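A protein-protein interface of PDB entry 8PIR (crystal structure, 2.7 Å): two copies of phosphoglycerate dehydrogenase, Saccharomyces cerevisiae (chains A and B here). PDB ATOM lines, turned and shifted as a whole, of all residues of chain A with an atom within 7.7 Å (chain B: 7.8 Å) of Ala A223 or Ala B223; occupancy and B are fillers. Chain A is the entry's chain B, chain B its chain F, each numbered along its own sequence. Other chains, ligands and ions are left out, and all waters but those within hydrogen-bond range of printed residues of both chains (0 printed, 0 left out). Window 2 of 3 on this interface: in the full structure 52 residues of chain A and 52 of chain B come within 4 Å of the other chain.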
ATOM      1  N   ARG A 161      10.765 -10.343  10.377  1.00  0.00           N
ATOM      2  CA  ARG A 161       9.737 -10.945   9.489  1.00  0.00           C
ATOM      3  C   ARG A 161       8.609  -9.933   9.277  1.00  0.00           C
ATOM      4  O   ARG A 161       8.148  -9.790   8.132  1.00  0.00           O
ATOM      5  CB  ARG A 161       9.196 -12.237  10.105  1.00  0.00           C
ATOM      6  CG  ARG A 161       8.113 -12.912   9.279  1.00  0.00           C
ATOM      7  CD  ARG A 161       8.577 -13.355   7.901  1.00  0.00           C
ATOM      8  NE  ARG A 161       7.440 -13.671   7.045  1.00  0.00           N
ATOM      9  CZ  ARG A 161       7.441 -14.585   6.085  1.00  0.00           C
ATOM     10  NH1 ARG A 161       8.539 -15.260   5.809  1.00  0.00           N
ATOM     11  NH2 ARG A 161       6.351 -14.789   5.365  1.00  0.00           N
ATOM     12  N   ILE A 168       6.942  -6.140   1.262  1.00  0.00           N
ATOM     13  CA  ILE A 168       6.298  -6.904   0.151  1.00  0.00           C
ATOM     14  C   ILE A 168       4.939  -6.264  -0.140  1.00  0.00           C
ATOM     15  O   ILE A 168       4.703  -5.869  -1.291  1.00  0.00           O
ATOM     16  CB  ILE A 168       6.159  -8.405   0.471  1.00  0.00           C
ATOM     17  CG1 ILE A 168       7.525  -9.092   0.593  1.00  0.00           C
ATOM     18  CG2 ILE A 168       5.280  -9.082  -0.575  1.00  0.00           C
ATOM     19  CD1 ILE A 168       8.282  -9.180  -0.714  1.00  0.00           C
ATOM     20  N   VAL A 200       4.776  -6.955 -10.161  1.00  0.00           N
ATOM     21  CA  VAL A 200       6.128  -6.972  -9.528  1.00  0.00           C
ATOM     22  C   VAL A 200       7.008  -7.980 -10.282  1.00  0.00           C
ATOM     23  O   VAL A 200       8.161  -7.659 -10.547  1.00  0.00           O
ATOM     24  CB  VAL A 200       6.056  -7.231  -8.009  1.00  0.00           C
ATOM     25  CG1 VAL A 200       5.139  -6.228  -7.326  1.00  0.00           C
ATOM     26  CG2 VAL A 200       5.633  -8.649  -7.665  1.00  0.00           C
ATOM     27  N   LEU A 217      13.822 -10.415   3.527  1.00  0.00           N
ATOM     28  CA  LEU A 217      13.125  -9.720   2.411  1.00  0.00           C
ATOM     29  C   LEU A 217      13.598 -10.306   1.076  1.00  0.00           C
ATOM     30  O   LEU A 217      12.754 -10.499   0.171  1.00  0.00           O
ATOM     31  CB  LEU A 217      13.412  -8.217   2.479  1.00  0.00           C
ATOM     32  CG  LEU A 217      12.783  -7.384   1.362  1.00  0.00           C
ATOM     33  CD1 LEU A 217      11.262  -7.488   1.388  1.00  0.00           C
ATOM     34  CD2 LEU A 217      13.204  -5.931   1.464  1.00  0.00           C
ATOM     35  N   SER A 218      14.909 -10.504   0.930  1.00  0.00           N
ATOM     36  CA  SER A 218      15.545 -11.051  -0.296  1.00  0.00           C
ATOM     37  C   SER A 218      14.772 -12.284  -0.767  1.00  0.00           C
ATOM     38  O   SER A 218      14.461 -12.363  -1.967  1.00  0.00           O
ATOM     39  CB  SER A 218      16.994 -11.383  -0.069  1.00  0.00           C
ATOM     40  OG  SER A 218      17.616 -11.725  -1.296  1.00  0.00           O
ATOM     41  N   VAL A 219      14.506 -13.217   0.149  1.00  0.00           N
ATOM     42  CA  VAL A 219      13.939 -14.560  -0.167  1.00  0.00           C
ATOM     43  C   VAL A 219      12.463 -14.401  -0.562  1.00  0.00           C
ATOM     44  O   VAL A 219      12.090 -14.927  -1.627  1.00  0.00           O
ATOM     45  CB  VAL A 219      14.127 -15.527   1.014  1.00  0.00           C
ATOM     46  CG1 VAL A 219      13.252 -16.766   0.890  1.00  0.00           C
ATOM     47  CG2 VAL A 219      15.584 -15.920   1.164  1.00  0.00           C
ATOM     48  N   LEU A 220      11.687 -13.623   0.203  1.00  0.00           N
ATOM     49  CA  LEU A 220      10.265 -13.296  -0.102  1.00  0.00           C
ATOM     50  C   LEU A 220      10.171 -12.660  -1.495  1.00  0.00           C
ATOM     51  O   LEU A 220       9.335 -13.122  -2.301  1.00  0.00           O
ATOM     52  CB  LEU A 220       9.703 -12.355   0.969  1.00  0.00           C
ATOM     53  CG  LEU A 220       9.580 -12.939   2.375  1.00  0.00           C
ATOM     54  CD1 LEU A 220       8.899 -11.952   3.314  1.00  0.00           C
ATOM     55  CD2 LEU A 220       8.822 -14.254   2.351  1.00  0.00           C
ATOM     56  N   ALA A 221      11.029 -11.679  -1.782  1.00  0.00           N
ATOM     57  CA  ALA A 221      11.036 -10.905  -3.047  1.00  0.00           C
ATOM     58  C   ALA A 221      11.305 -11.833  -4.245  1.00  0.00           C
ATOM     59  O   ALA A 221      10.696 -11.619  -5.322  1.00  0.00           O
ATOM     60  CB  ALA A 221      12.058  -9.802  -2.957  1.00  0.00           C
ATOM     61  N   GLU A 222      12.233 -12.783  -4.102  1.00  0.00           N
ATOM     62  CA  GLU A 222      12.572 -13.759  -5.176  1.00  0.00           C
ATOM     63  C   GLU A 222      11.348 -14.643  -5.436  1.00  0.00           C
ATOM     64  O   GLU A 222      10.952 -14.791  -6.610  1.00  0.00           O
ATOM     65  CB  GLU A 222      13.785 -14.609  -4.793  1.00  0.00           C
ATOM     66  CG  GLU A 222      15.103 -13.895  -5.012  1.00  0.00           C
ATOM     67  CD  GLU A 222      16.280 -14.800  -5.320  1.00  0.00           C
ATOM     68  OE1 GLU A 222      16.442 -15.844  -4.639  1.00  0.00           O
ATOM     69  OE2 GLU A 222      17.041 -14.451  -6.241  1.00  0.00           O
ATOM     70  N   ALA A 223      10.704 -15.094  -4.359  1.00  0.00           N
ATOM     71  CA  ALA A 223       9.492 -15.940  -4.394  1.00  0.00           C
ATOM     72  C   ALA A 223       8.321 -15.180  -5.043  1.00  0.00           C
ATOM     73  O   ALA A 223       7.529 -15.836  -5.735  1.00  0.00           O
ATOM     74  CB  ALA A 223       9.179 -16.401  -2.996  1.00  0.00           C
ATOM     75  N   MET A 224       8.271 -13.846  -4.927  1.00  0.00           N
ATOM     76  CA  MET A 224       7.273 -12.984  -5.623  1.00  0.00           C
ATOM     77  C   MET A 224       7.742 -12.647  -7.043  1.00  0.00           C
ATOM     78  O   MET A 224       7.060 -11.829  -7.700  1.00  0.00           O
ATOM     79  CB  MET A 224       7.032 -11.673  -4.865  1.00  0.00           C
ATOM     80  CG  MET A 224       6.376 -11.868  -3.506  1.00  0.00           C
ATOM     81  SD  MET A 224       4.783 -12.740  -3.592  1.00  0.00           S
ATOM     82  CE  MET A 224       3.864 -11.620  -4.647  1.00  0.00           C
ATOM     83  N   GLY A 225       8.912 -13.151  -7.447  1.00  0.00           N
ATOM     84  CA  GLY A 225       9.398 -13.097  -8.838  1.00  0.00           C
ATOM     85  C   GLY A 225      10.152 -11.810  -9.134  1.00  0.00           C
ATOM     86  O   GLY A 225      10.222 -11.431 -10.320  1.00  0.00           O
ATOM     87  N   LEU A 226      10.738 -11.182  -8.112  1.00  0.00           N
ATOM     88  CA  LEU A 226      11.635 -10.011  -8.287  1.00  0.00           C
ATOM     89  C   LEU A 226      13.083 -10.493  -8.392  1.00  0.00           C
ATOM     90  O   LEU A 226      13.440 -11.479  -7.698  1.00  0.00           O
ATOM     91  CB  LEU A 226      11.456  -9.050  -7.109  1.00  0.00           C
ATOM     92  CG  LEU A 226      10.098  -8.367  -7.021  1.00  0.00           C
ATOM     93  CD1 LEU A 226       9.975  -7.585  -5.731  1.00  0.00           C
ATOM     94  CD2 LEU A 226       9.874  -7.452  -8.208  1.00  0.00           C
ATOM     95  N   VAL A 228      16.686  -9.468  -7.245  1.00  0.00           N
ATOM     96  CA  VAL A 228      17.226  -8.777  -6.034  1.00  0.00           C
ATOM     97  C   VAL A 228      18.686  -8.378  -6.285  1.00  0.00           C
ATOM     98  O   VAL A 228      19.534  -9.277  -6.406  1.00  0.00           O
ATOM     99  CB  VAL A 228      17.114  -9.672  -4.788  1.00  0.00           C
ATOM    100  CG1 VAL A 228      17.707  -8.997  -3.562  1.00  0.00           C
ATOM    101  CG2 VAL A 228      15.679 -10.095  -4.525  1.00  0.00           C
ATOM    102  N   ARG B 161      -2.013 -13.466 -13.327  1.00  0.00           N
ATOM    103  CA  ARG B 161      -0.859 -13.103 -12.466  1.00  0.00           C
ATOM    104  C   ARG B 161      -1.171 -11.762 -11.793  1.00  0.00           C
ATOM    105  O   ARG B 161      -0.880 -11.626 -10.587  1.00  0.00           O
ATOM    106  CB  ARG B 161       0.420 -13.045 -13.308  1.00  0.00           C
ATOM    107  CG  ARG B 161       1.647 -12.570 -12.548  1.00  0.00           C
ATOM    108  CD  ARG B 161       2.081 -13.507 -11.438  1.00  0.00           C
ATOM    109  NE  ARG B 161       3.053 -12.856 -10.561  1.00  0.00           N
ATOM    110  CZ  ARG B 161       3.998 -13.489  -9.881  1.00  0.00           C
ATOM    111  NH1 ARG B 161       4.126 -14.801  -9.971  1.00  0.00           N
ATOM    112  NH2 ARG B 161       4.786 -12.809  -9.069  1.00  0.00           N
ATOM    113  N   ILE B 168      -2.309 -11.051  -2.863  1.00  0.00           N
ATOM    114  CA  ILE B 168      -1.154 -11.102  -1.913  1.00  0.00           C
ATOM    115  C   ILE B 168      -1.035  -9.736  -1.232  1.00  0.00           C
ATOM    116  O   ILE B 168      -1.082  -9.684   0.006  1.00  0.00           O
ATOM    117  CB  ILE B 168       0.156 -11.497  -2.625  1.00  0.00           C
ATOM    118  CG1 ILE B 168       0.110 -12.933  -3.147  1.00  0.00           C
ATOM    119  CG2 ILE B 168       1.347 -11.279  -1.702  1.00  0.00           C
ATOM    120  CD1 ILE B 168       0.052 -13.985  -2.048  1.00  0.00           C
ATOM    121  N   VAL B 200       1.520 -12.783   8.090  1.00  0.00           N
ATOM    122  CA  VAL B 200       0.793 -13.747   7.232  1.00  0.00           C
ATOM    123  C   VAL B 200       1.381 -15.141   7.475  1.00  0.00           C
ATOM    124  O   VAL B 200       0.627 -16.076   7.528  1.00  0.00           O
ATOM    125  CB  VAL B 200       0.786 -13.284   5.767  1.00  0.00           C
ATOM    126  CG1 VAL B 200       0.302 -11.849   5.647  1.00  0.00           C
ATOM    127  CG2 VAL B 200       2.130 -13.449   5.083  1.00  0.00           C
ATOM    128  N   ARG B 201       2.674 -15.253   7.736  1.00  0.00           N
ATOM    129  CA  ARG B 201       3.276 -16.593   7.901  1.00  0.00           C
ATOM    130  C   ARG B 201       2.559 -17.340   9.021  1.00  0.00           C
ATOM    131  O   ARG B 201       2.415 -16.767  10.094  1.00  0.00           O
ATOM    132  CB  ARG B 201       4.765 -16.438   8.202  1.00  0.00           C
ATOM    133  CG  ARG B 201       5.543 -17.741   8.259  1.00  0.00           C
ATOM    134  CD  ARG B 201       6.997 -17.465   8.577  1.00  0.00           C
ATOM    135  NE  ARG B 201       7.165 -16.909   9.910  1.00  0.00           N
ATOM    136  CZ  ARG B 201       8.326 -16.515  10.410  1.00  0.00           C
ATOM    137  NH1 ARG B 201       9.423 -16.606   9.681  1.00  0.00           N
ATOM    138  NH2 ARG B 201       8.386 -16.025  11.633  1.00  0.00           N
ATOM    139  N   LEU B 217      -2.161 -18.131  -7.394  1.00  0.00           N
ATOM    140  CA  LEU B 217      -2.243 -17.574  -6.018  1.00  0.00           C
ATOM    141  C   LEU B 217      -1.723 -18.600  -5.002  1.00  0.00           C
ATOM    142  O   LEU B 217      -1.014 -18.195  -4.056  1.00  0.00           O
ATOM    143  CB  LEU B 217      -3.693 -17.190  -5.720  1.00  0.00           C
ATOM    144  CG  LEU B 217      -3.925 -16.604  -4.330  1.00  0.00           C
ATOM    145  CD1 LEU B 217      -3.107 -15.332  -4.122  1.00  0.00           C
ATOM    146  CD2 LEU B 217      -5.401 -16.346  -4.104  1.00  0.00           C
ATOM    147  N   SER B 218      -2.109 -19.868  -5.153  1.00  0.00           N
ATOM    148  CA  SER B 218      -1.674 -20.988  -4.276  1.00  0.00           C
ATOM    149  C   SER B 218      -0.160 -20.929  -4.062  1.00  0.00           C
ATOM    150  O   SER B 218       0.282 -21.041  -2.904  1.00  0.00           O
ATOM    151  CB  SER B 218      -2.070 -22.316  -4.843  1.00  0.00           C
ATOM    152  OG  SER B 218      -1.826 -23.349  -3.899  1.00  0.00           O
ATOM    153  N   VAL B 219       0.599 -20.776  -5.148  1.00  0.00           N
ATOM    154  CA  VAL B 219       2.088 -20.870  -5.162  1.00  0.00           C
ATOM    155  C   VAL B 219       2.683 -19.634  -4.468  1.00  0.00           C
ATOM    156  O   VAL B 219       3.506 -19.816  -3.548  1.00  0.00           O
ATOM    157  CB  VAL B 219       2.605 -21.046  -6.605  1.00  0.00           C
ATOM    158  CG1 VAL B 219       4.093 -20.759  -6.730  1.00  0.00           C
ATOM    159  CG2 VAL B 219       2.270 -22.429  -7.141  1.00  0.00           C
ATOM    160  N   LEU B 220       2.203 -18.435  -4.814  1.00  0.00           N
ATOM    161  CA  LEU B 220       2.603 -17.151  -4.170  1.00  0.00           C
ATOM    162  C   LEU B 220       2.334 -17.222  -2.661  1.00  0.00           C
ATOM    163  O   LEU B 220       3.245 -16.888  -1.882  1.00  0.00           O
ATOM    164  CB  LEU B 220       1.837 -15.990  -4.814  1.00  0.00           C
ATOM    165  CG  LEU B 220       2.179 -15.722  -6.276  1.00  0.00           C
ATOM    166  CD1 LEU B 220       1.439 -14.505  -6.799  1.00  0.00           C
ATOM    167  CD2 LEU B 220       3.679 -15.545  -6.455  1.00  0.00           C
ATOM    168  N   ALA B 221       1.148 -17.688  -2.264  1.00  0.00           N
ATOM    169  CA  ALA B 221       0.712 -17.777  -0.852  1.00  0.00           C
ATOM    170  C   ALA B 221       1.660 -18.691  -0.060  1.00  0.00           C
ATOM    171  O   ALA B 221       1.956 -18.374   1.111  1.00  0.00           O
ATOM    172  CB  ALA B 221      -0.710 -18.276  -0.786  1.00  0.00           C
ATOM    173  N   GLU B 222       2.048 -19.833  -0.629  1.00  0.00           N
ATOM    174  CA  GLU B 222       2.943 -20.805   0.058  1.00  0.00           C
ATOM    175  C   GLU B 222       4.326 -20.170   0.237  1.00  0.00           C
ATOM    176  O   GLU B 222       4.850 -20.203   1.367  1.00  0.00           O
ATOM    177  CB  GLU B 222       3.010 -22.121  -0.710  1.00  0.00           C
ATOM    178  CG  GLU B 222       1.799 -23.005  -0.466  1.00  0.00           C
ATOM    179  CD  GLU B 222       2.041 -24.490  -0.659  1.00  0.00           C
ATOM    180  OE1 GLU B 222       2.630 -24.855  -1.687  1.00  0.00           O
ATOM    181  OE2 GLU B 222       1.604 -25.282   0.203  1.00  0.00           O
ATOM    182  N   ALA B 223       4.791 -19.446  -0.783  1.00  0.00           N
ATOM    183  CA  ALA B 223       6.054 -18.670  -0.771  1.00  0.00           C
ATOM    184  C   ALA B 223       6.017 -17.577   0.307  1.00  0.00           C
ATOM    185  O   ALA B 223       7.067 -17.329   0.912  1.00  0.00           O
ATOM    186  CB  ALA B 223       6.303 -18.091  -2.140  1.00  0.00           C
ATOM    187  N   MET B 224       4.856 -16.967   0.573  1.00  0.00           N
ATOM    188  CA  MET B 224       4.690 -15.946   1.649  1.00  0.00           C
ATOM    189  C   MET B 224       4.397 -16.645   2.983  1.00  0.00           C
ATOM    190  O   MET B 224       4.173 -15.937   3.975  1.00  0.00           O
ATOM    191  CB  MET B 224       3.555 -14.966   1.346  1.00  0.00           C
ATOM    192  CG  MET B 224       3.775 -14.150   0.081  1.00  0.00           C
ATOM    193  SD  MET B 224       5.270 -13.114   0.100  1.00  0.00           S
ATOM    194  CE  MET B 224       4.927 -12.071   1.515  1.00  0.00           C
ATOM    195  N   GLY B 225       4.394 -17.981   3.005  1.00  0.00           N
ATOM    196  CA  GLY B 225       4.419 -18.776   4.248  1.00  0.00           C
ATOM    197  C   GLY B 225       3.021 -19.078   4.754  1.00  0.00           C
ATOM    198  O   GLY B 225       2.865 -19.327   5.967  1.00  0.00           O
ATOM    199  N   LEU B 226       2.030 -19.066   3.859  1.00  0.00           N
ATOM    200  CA  LEU B 226       0.626 -19.405   4.191  1.00  0.00           C
ATOM    201  C   LEU B 226       0.392 -20.883   3.881  1.00  0.00           C
ATOM    202  O   LEU B 226       0.968 -21.373   2.896  1.00  0.00           O
ATOM    203  CB  LEU B 226      -0.318 -18.501   3.391  1.00  0.00           C
ATOM    204  CG  LEU B 226      -0.274 -17.018   3.760  1.00  0.00           C
ATOM    205  CD1 LEU B 226      -1.104 -16.182   2.807  1.00  0.00           C
ATOM    206  CD2 LEU B 226      -0.762 -16.807   5.180  1.00  0.00           C
ATOM    207  N   VAL B 228      -2.389 -23.259   2.446  1.00  0.00           N
ATOM    208  CA  VAL B 228      -3.457 -23.113   1.411  1.00  0.00           C
ATOM    209  C   VAL B 228      -4.411 -24.305   1.522  1.00  0.00           C
ATOM    210  O   VAL B 228      -3.975 -25.447   1.267  1.00  0.00           O
ATOM    211  CB  VAL B 228      -2.851 -23.028   0.002  1.00  0.00           C
ATOM    212  CG1 VAL B 228      -3.913 -23.002  -1.075  1.00  0.00           C
ATOM    213  CG2 VAL B 228      -1.930 -21.835  -0.135  1.00  0.00           C
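Of the 14 printed residues of chain A, 5 touch a printed residue of chain B. Printed residues of chain B that touch a printed residue of chain A: Arg B161, Ile B168, Arg B201, Leu B220, Ala B223 and Met B224. Hydrophobic or aromatic side chains of chain B that line the printed part of chain A: Ile B168, Leu B220, Ala B223 and Met B224. Along chain B the printed residues that touch a printed residue of chain A span positions 161 to 224. Among the printed residues, no Asp or Glu carboxylate lies within 4 Å of a Lys or Arg side-chain nitrogen of the other chain.
Arg A161 touches Met B224, and with the chains exchanged Met A224 touches Arg B161. Ile A168 touches Met B224, and with the chains exchanged Met A224 touches Ile B168. Ala A223 touches its own counterpart, Ala B223. Met A224 touches its own counterpart, Met B224. 14 positions are printed for both chains.
Of chain B, only Leu B220 (3.9 Å) and Ala B223 (3.4 Å) come within 4 Å of Ala A223. Ala B223 touches just these residues of chain A: Leu A220 and Ala A223. Of the printed residues of chain B, Ile A168 touches Met B224 (3.7 Å). Printed residues of chain A within 4 Å of Ile B168: Met A224 (3.9 Å). Of the printed residues of chain A, Leu B220 touches Ala A223 (3.9 Å). Gly B225 touches none of the printed residues of chain A. The nearest residue of chain B that does not touch Ala A223 is Arg B161 (5.3 Å). The nearest residue of chain A that does not touch Ala B223 is Arg A161 (5.2 Å).
Among the printed residues, pairs that only touch across the chains: Arg A161 with Arg B201, Ile A168 with Met B224, Leu A220 with Ala B223, Ala A223 with Leu B220, Ala A223 with Ala B223 and Met A224 with Ile B168.
The backbone carbonyl oxygen (O) of Met A224 lies within hydrogen-bond range of the guanidinium group (NH2) of Arg B161, 2.8 Å away. The backbone carbonyl oxygen of Met B224 sits at hydrogen-bond distance from the guanidinium group of Arg A161. SD of Met A224 sits close to SD of Met B224 (3.7 Å).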
